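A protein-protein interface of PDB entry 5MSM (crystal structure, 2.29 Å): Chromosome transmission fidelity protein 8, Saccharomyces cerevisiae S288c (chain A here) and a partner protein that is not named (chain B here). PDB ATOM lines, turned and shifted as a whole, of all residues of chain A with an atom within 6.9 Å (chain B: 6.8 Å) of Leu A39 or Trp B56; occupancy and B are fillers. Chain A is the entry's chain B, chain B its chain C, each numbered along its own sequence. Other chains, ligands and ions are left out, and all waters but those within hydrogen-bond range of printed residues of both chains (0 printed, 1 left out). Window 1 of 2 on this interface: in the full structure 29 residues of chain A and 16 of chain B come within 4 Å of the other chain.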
ATOM      1  N   LEU A  33     -21.923   4.940  32.584  1.00  0.00           N
ATOM      2  CA  LEU A  33     -22.662   4.971  31.337  1.00  0.00           C
ATOM      3  C   LEU A  33     -22.821   3.568  30.748  1.00  0.00           C
ATOM      4  O   LEU A  33     -21.826   2.866  30.537  1.00  0.00           O
ATOM      5  CB  LEU A  33     -21.936   5.875  30.341  1.00  0.00           C
ATOM      6  CG  LEU A  33     -22.425   5.793  28.906  1.00  0.00           C
ATOM      7  CD1 LEU A  33     -23.886   6.270  28.875  1.00  0.00           C
ATOM      8  CD2 LEU A  33     -21.534   6.633  27.999  1.00  0.00           C
ATOM      9  N   ILE A  35     -24.572   1.014  27.697  1.00  0.00           N
ATOM     10  CA  ILE A  35     -25.149   0.952  26.359  1.00  0.00           C
ATOM     11  C   ILE A  35     -25.311  -0.484  25.897  1.00  0.00           C
ATOM     12  O   ILE A  35     -24.379  -1.273  26.010  1.00  0.00           O
ATOM     13  CB  ILE A  35     -24.254   1.699  25.344  1.00  0.00           C
ATOM     14  CG1 ILE A  35     -24.056   3.167  25.748  1.00  0.00           C
ATOM     15  CG2 ILE A  35     -24.799   1.582  23.954  1.00  0.00           C
ATOM     16  CD1 ILE A  35     -22.803   3.789  25.146  1.00  0.00           C
ATOM     17  N   GLY A  37     -24.765  -2.396  23.308  1.00  0.00           N
ATOM     18  CA  GLY A  37     -24.070  -2.441  22.038  1.00  0.00           C
ATOM     19  C   GLY A  37     -22.592  -2.168  22.220  1.00  0.00           C
ATOM     20  O   GLY A  37     -22.127  -1.938  23.339  1.00  0.00           O
ATOM     21  N   GLU A  38     -21.849  -2.186  21.124  1.00  0.00           N
ATOM     22  CA  GLU A  38     -20.446  -1.809  21.154  1.00  0.00           C
ATOM     23  C   GLU A  38     -20.280  -0.347  20.719  1.00  0.00           C
ATOM     24  O   GLU A  38     -20.833   0.080  19.718  1.00  0.00           O
ATOM     25  CB  GLU A  38     -19.626  -2.694  20.216  1.00  0.00           C
ATOM     26  CG  GLU A  38     -19.939  -4.158  20.323  1.00  0.00           C
ATOM     27  CD  GLU A  38     -18.766  -4.978  20.817  1.00  0.00           C
ATOM     28  OE1 GLU A  38     -17.599  -4.535  20.657  1.00  0.00           O
ATOM     29  OE2 GLU A  38     -19.025  -6.071  21.379  1.00  0.00           O
ATOM     30  N   LEU A  39     -19.473   0.398  21.452  1.00  0.00           N
ATOM     31  CA  LEU A  39     -19.079   1.721  21.042  1.00  0.00           C
ATOM     32  C   LEU A  39     -17.886   1.589  20.117  1.00  0.00           C
ATOM     33  O   LEU A  39     -16.834   1.106  20.531  1.00  0.00           O
ATOM     34  CB  LEU A  39     -18.727   2.570  22.254  1.00  0.00           C
ATOM     35  CG  LEU A  39     -18.203   3.953  21.899  1.00  0.00           C
ATOM     36  CD1 LEU A  39     -19.268   4.703  21.123  1.00  0.00           C
ATOM     37  CD2 LEU A  39     -17.851   4.714  23.145  1.00  0.00           C
ATOM     38  N   GLU A  40     -18.060   1.982  18.859  1.00  0.00           N
ATOM     39  CA  GLU A  40     -17.012   1.841  17.852  1.00  0.00           C
ATOM     40  C   GLU A  40     -16.217   3.116  17.709  1.00  0.00           C
ATOM     41  O   GLU A  40     -16.657   4.072  17.073  1.00  0.00           O
ATOM     42  CB  GLU A  40     -17.596   1.450  16.487  1.00  0.00           C
ATOM     43  CG  GLU A  40     -18.381   0.120  16.454  1.00  0.00           C
ATOM     44  CD  GLU A  40     -17.507  -1.130  16.647  1.00  0.00           C
ATOM     45  OE1 GLU A  40     -16.273  -1.053  16.457  1.00  0.00           O
ATOM     46  OE2 GLU A  40     -18.059  -2.201  16.978  1.00  0.00           O
ATOM     47  N   LEU A  41     -15.024   3.117  18.281  1.00  0.00           N
ATOM     48  CA  LEU A  41     -14.129   4.249  18.162  1.00  0.00           C
ATOM     49  C   LEU A  41     -13.019   3.833  17.239  1.00  0.00           C
ATOM     50  O   LEU A  41     -12.768   2.642  17.065  1.00  0.00           O
ATOM     51  CB  LEU A  41     -13.585   4.657  19.526  1.00  0.00           C
ATOM     52  CG  LEU A  41     -14.673   4.822  20.567  1.00  0.00           C
ATOM     53  CD1 LEU A  41     -14.080   5.282  21.875  1.00  0.00           C
ATOM     54  CD2 LEU A  41     -15.673   5.822  20.010  1.00  0.00           C
ATOM     55  N   PRO A  42     -12.339   4.811  16.645  1.00  0.00           N
ATOM     56  CA  PRO A  42     -11.280   4.451  15.705  1.00  0.00           C
ATOM     57  C   PRO A  42     -10.121   3.752  16.406  1.00  0.00           C
ATOM     58  O   PRO A  42      -9.874   4.025  17.584  1.00  0.00           O
ATOM     59  CB  PRO A  42     -10.835   5.799  15.127  1.00  0.00           C
ATOM     60  CG  PRO A  42     -11.774   6.835  15.657  1.00  0.00           C
ATOM     61  CD  PRO A  42     -12.469   6.265  16.837  1.00  0.00           C
ATOM     62  N   PHE A  70     -16.614  11.726  21.762  1.00  0.00           N
ATOM     63  CA  PHE A  70     -17.425  10.794  20.977  1.00  0.00           C
ATOM     64  C   PHE A  70     -18.935  11.062  20.999  1.00  0.00           C
ATOM     65  O   PHE A  70     -19.662  10.542  20.140  1.00  0.00           O
ATOM     66  CB  PHE A  70     -17.135   9.334  21.400  1.00  0.00           C
ATOM     67  CG  PHE A  70     -17.659   8.952  22.772  1.00  0.00           C
ATOM     68  CD1 PHE A  70     -18.974   8.541  22.952  1.00  0.00           C
ATOM     69  CD2 PHE A  70     -16.821   8.954  23.871  1.00  0.00           C
ATOM     70  CE1 PHE A  70     -19.438   8.166  24.192  1.00  0.00           C
ATOM     71  CE2 PHE A  70     -17.292   8.588  25.117  1.00  0.00           C
ATOM     72  CZ  PHE A  70     -18.596   8.194  25.281  1.00  0.00           C
ATOM     73  N   LEU A  82     -28.598  10.380  24.260  1.00  0.00           N
ATOM     74  CA  LEU A  82     -27.198  10.218  23.963  1.00  0.00           C
ATOM     75  C   LEU A  82     -27.003  10.474  22.479  1.00  0.00           C
ATOM     76  O   LEU A  82     -27.670   9.854  21.658  1.00  0.00           O
ATOM     77  CB  LEU A  82     -26.741   8.815  24.352  1.00  0.00           C
ATOM     78  CG  LEU A  82     -25.316   8.430  23.969  1.00  0.00           C
ATOM     79  CD1 LEU A  82     -24.387   9.290  24.792  1.00  0.00           C
ATOM     80  CD2 LEU A  82     -25.013   6.926  24.176  1.00  0.00           C
ATOM     81  N   VAL A  84     -24.335  10.140  19.554  1.00  0.00           N
ATOM     82  CA  VAL A  84     -23.047   9.578  19.289  1.00  0.00           C
ATOM     83  C   VAL A  84     -22.590   9.875  17.882  1.00  0.00           C
ATOM     84  O   VAL A  84     -23.285   9.538  16.902  1.00  0.00           O
ATOM     85  CB  VAL A  84     -23.036   8.071  19.528  1.00  0.00           C
ATOM     86  CG1 VAL A  84     -21.694   7.496  19.109  1.00  0.00           C
ATOM     87  CG2 VAL A  84     -23.317   7.789  20.991  1.00  0.00           C
ATOM     88  N   GLY A  85     -21.388  10.452  17.789  1.00  0.00           N
ATOM     89  CA  GLY A  85     -20.830  10.851  16.519  1.00  0.00           C
ATOM     90  C   GLY A  85     -21.800  11.833  15.878  1.00  0.00           C
ATOM     91  O   GLY A  85     -22.513  12.550  16.584  1.00  0.00           O
ATOM     92  N   LYS A  86     -21.869  11.834  14.551  1.00  0.00           N
ATOM     93  CA  LYS A  86     -22.656  12.829  13.841  1.00  0.00           C
ATOM     94  C   LYS A  86     -24.064  12.347  13.565  1.00  0.00           C
ATOM     95  O   LYS A  86     -24.967  13.151  13.338  1.00  0.00           O
ATOM     96  CB  LYS A  86     -21.976  13.206  12.525  1.00  0.00           C
ATOM     97  CG  LYS A  86     -20.469  13.026  12.541  1.00  0.00           C
ATOM     98  CD  LYS A  86     -19.798  13.735  11.359  1.00  0.00           C
ATOM     99  CE  LYS A  86     -18.283  13.470  11.344  1.00  0.00           C
ATOM    100  NZ  LYS A  86     -17.614  13.944  10.090  1.00  0.00           N
ATOM    101  N   LYS A  87     -24.274  11.040  13.591  1.00  0.00           N
ATOM    102  CA  LYS A  87     -25.452  10.505  12.927  1.00  0.00           C
ATOM    103  C   LYS A  87     -26.389   9.696  13.808  1.00  0.00           C
ATOM    104  O   LYS A  87     -27.325   9.075  13.305  1.00  0.00           O
ATOM    105  CB  LYS A  87     -24.984   9.654  11.744  1.00  0.00           C
ATOM    106  CG  LYS A  87     -24.488  10.497  10.582  1.00  0.00           C
ATOM    107  CD  LYS A  87     -23.572   9.711   9.671  1.00  0.00           C
ATOM    108  CE  LYS A  87     -22.924  10.637   8.644  1.00  0.00           C
ATOM    109  NZ  LYS A  87     -21.801   9.969   7.914  1.00  0.00           N
ATOM    110  N   GLN A  88     -26.159   9.688  15.115  1.00  0.00           N
ATOM    111  CA  GLN A  88     -26.946   8.801  15.955  1.00  0.00           C
ATOM    112  C   GLN A  88     -27.521   9.454  17.190  1.00  0.00           C
ATOM    113  O   GLN A  88     -26.870  10.241  17.859  1.00  0.00           O
ATOM    114  CB  GLN A  88     -26.099   7.594  16.397  1.00  0.00           C
ATOM    115  CG  GLN A  88     -25.924   6.513  15.359  1.00  0.00           C
ATOM    116  CD  GLN A  88     -25.229   5.282  15.941  1.00  0.00           C
ATOM    117  OE1 GLN A  88     -24.456   5.386  16.898  1.00  0.00           O
ATOM    118  NE2 GLN A  88     -25.509   4.112  15.366  1.00  0.00           N
ATOM    119  N   LYS B  54     -15.256   8.680  11.970  1.00  0.00           N
ATOM    120  CA  LYS B  54     -16.609   8.181  12.083  1.00  0.00           C
ATOM    121  C   LYS B  54     -16.869   7.435  13.409  1.00  0.00           C
ATOM    122  O   LYS B  54     -16.204   6.457  13.727  1.00  0.00           O
ATOM    123  CB  LYS B  54     -16.975   7.313  10.878  1.00  0.00           C
ATOM    124  CG  LYS B  54     -18.460   7.086  10.927  1.00  0.00           C
ATOM    125  CD  LYS B  54     -19.093   8.485  11.123  1.00  0.00           C
ATOM    126  CE  LYS B  54     -20.593   8.467  11.288  1.00  0.00           C
ATOM    127  NZ  LYS B  54     -21.001   7.713  12.493  1.00  0.00           N
ATOM    128  N   ILE B  55     -17.853   7.915  14.171  1.00  0.00           N
ATOM    129  CA  ILE B  55     -18.156   7.375  15.495  1.00  0.00           C
ATOM    130  C   ILE B  55     -19.605   6.895  15.671  1.00  0.00           C
ATOM    131  O   ILE B  55     -20.556   7.654  15.420  1.00  0.00           O
ATOM    132  CB  ILE B  55     -17.869   8.431  16.580  1.00  0.00           C
ATOM    133  CG1 ILE B  55     -16.415   8.881  16.514  1.00  0.00           C
ATOM    134  CG2 ILE B  55     -18.174   7.871  17.936  1.00  0.00           C
ATOM    135  CD1 ILE B  55     -16.178  10.204  17.179  1.00  0.00           C
ATOM    136  N   TRP B  56     -19.772   5.645  16.115  1.00  0.00           N
ATOM    137  CA  TRP B  56     -21.119   5.079  16.267  1.00  0.00           C
ATOM    138  C   TRP B  56     -21.273   3.917  17.278  1.00  0.00           C
ATOM    139  O   TRP B  56     -20.294   3.272  17.688  1.00  0.00           O
ATOM    140  CB  TRP B  56     -21.619   4.628  14.877  1.00  0.00           C
ATOM    141  CG  TRP B  56     -20.995   3.374  14.350  1.00  0.00           C
ATOM    142  CD1 TRP B  56     -21.533   2.122  14.378  1.00  0.00           C
ATOM    143  CD2 TRP B  56     -19.713   3.244  13.711  1.00  0.00           C
ATOM    144  NE1 TRP B  56     -20.668   1.211  13.798  1.00  0.00           N
ATOM    145  CE2 TRP B  56     -19.543   1.875  13.383  1.00  0.00           C
ATOM    146  CE3 TRP B  56     -18.692   4.144  13.391  1.00  0.00           C
ATOM    147  CZ2 TRP B  56     -18.394   1.388  12.754  1.00  0.00           C
ATOM    148  CZ3 TRP B  56     -17.549   3.657  12.762  1.00  0.00           C
ATOM    149  CH2 TRP B  56     -17.412   2.286  12.453  1.00  0.00           C
ATOM    150  N   VAL B  57     -22.524   3.661  17.666  1.00  0.00           N
ATOM    151  CA  VAL B  57     -22.901   2.455  18.398  1.00  0.00           C
ATOM    152  C   VAL B  57     -23.388   1.361  17.455  1.00  0.00           C
ATOM    153  O   VAL B  57     -24.397   1.545  16.763  1.00  0.00           O
ATOM    154  CB  VAL B  57     -24.024   2.746  19.413  1.00  0.00           C
ATOM    155  CG1 VAL B  57     -24.624   1.459  19.954  1.00  0.00           C
ATOM    156  CG2 VAL B  57     -23.508   3.610  20.540  1.00  0.00           C
ATOM    157  N   LYS B  58     -22.702   0.219  17.439  1.00  0.00           N
ATOM    158  CA  LYS B  58     -23.272  -0.973  16.815  1.00  0.00           C
ATOM    159  C   LYS B  58     -24.165  -1.645  17.841  1.00  0.00           C
ATOM    160  O   LYS B  58     -23.682  -2.243  18.799  1.00  0.00           O
ATOM    161  CB  LYS B  58     -22.219  -1.973  16.342  1.00  0.00           C
ATOM    162  CG  LYS B  58     -22.871  -3.277  15.895  1.00  0.00           C
ATOM    163  CD  LYS B  58     -22.132  -4.508  16.371  1.00  0.00           C
ATOM    164  CE  LYS B  58     -23.098  -5.694  16.536  1.00  0.00           C
ATOM    165  NZ  LYS B  58     -23.774  -6.068  15.247  1.00  0.00           N
ATOM    166  N   TYR B  59     -25.466  -1.526  17.639  1.00  0.00           N
ATOM    167  CA  TYR B  59     -26.465  -2.025  18.565  1.00  0.00           C
ATOM    168  C   TYR B  59     -26.435  -3.541  18.762  1.00  0.00           C
ATOM    169  O   TYR B  59     -26.243  -4.290  17.815  1.00  0.00           O
ATOM    170  CB  TYR B  59     -27.848  -1.571  18.091  1.00  0.00           C
ATOM    171  CG  TYR B  59     -28.980  -1.847  19.052  1.00  0.00           C
ATOM    172  CD1 TYR B  59     -28.990  -1.289  20.311  1.00  0.00           C
ATOM    173  CD2 TYR B  59     -30.067  -2.635  18.678  1.00  0.00           C
ATOM    174  CE1 TYR B  59     -30.029  -1.520  21.186  1.00  0.00           C
ATOM    175  CE2 TYR B  59     -31.109  -2.875  19.557  1.00  0.00           C
ATOM    176  CZ  TYR B  59     -31.082  -2.304  20.807  1.00  0.00           C
ATOM    177  OH  TYR B  59     -32.117  -2.505  21.695  1.00  0.00           O
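N of Lys B58 sits at hydrogen-bond distance from O of Glu A38, at 3.0 Å. The backbone NH (N) of Glu A40 is in hydrogen-bond range of the backbone carbonyl oxygen (O) of Trp B56 (2.8 Å). The side-chain amide oxygen (OE1) of Gln A88 lies within hydrogen-bond range of the backbone NH (N) of Val B57 (2.7 Å).
The backbone carbonyl oxygen (O) of Phe A70 is in hydrogen-bond range of the backbone NH (N) of Gly A85, 2.9 Å away.
Gly A37 touches Lys B58. Glu A38 touches Trp B56 (O to O, 3.8 Å). O of Glu A38 touches CA of Val B57, at 3.4 Å. Ile B55 touches Glu A40. CD2 of Leu A41 touches CG2 of Ile B55 (3.8 Å). Ile B55 touches Phe A70. Ile B55 touches Val A84 (O to O, 3.6 Å). Val A84 touches Trp B56 (CG1 to CA, 3.8 Å). Ile B55 touches Gly A85 (O to CA, 3.4 Å). Lys B54 touches Lys A87.
Leu A39 touches just one residue of chain B: Trp B56 (3.8 Å). Of the printed residues of chain B, Leu A41 touches Ile B55 (3.8 Å). Leu A82 touches none of the printed residues of chain B. Printed residues of chain A within 4 Å of Lys B54: Lys A87. Trp B56 touches just these residues of chain A: Glu A38 (3.8 Å), Leu A39 (3.8 Å), Glu A40 (2.8 Å), Val A84 (3.8 Å) and Gln A88 (3.4 Å). Of the printed residues of chain A, Val B57 touches Glu A38 and Gln A88. The nearest residue of chain B that does not touch Leu A39 is Val B57 (4.4 Å). The nearest printed residue of chain A that does not touch Trp B56 is Leu A41 (5.3 Å).
Of the 6 printed residues of chain B, 5 touch a printed residue of chain A. Printed residues of chain B that touch a printed residue of chain A: Lys B54, Ile B55, Trp B56, Val B57 and Lys B58. Of the 15 printed residues of chain A, 10 touch a printed residue of chain B. Hydrophobic or aromatic side chains of chain A within 4 Å of the printed part of chain B: Leu A39, Leu A41, Phe A70 and Val A84. Along chain A the printed residues that touch a printed residue of chain B span positions 37 to 88.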
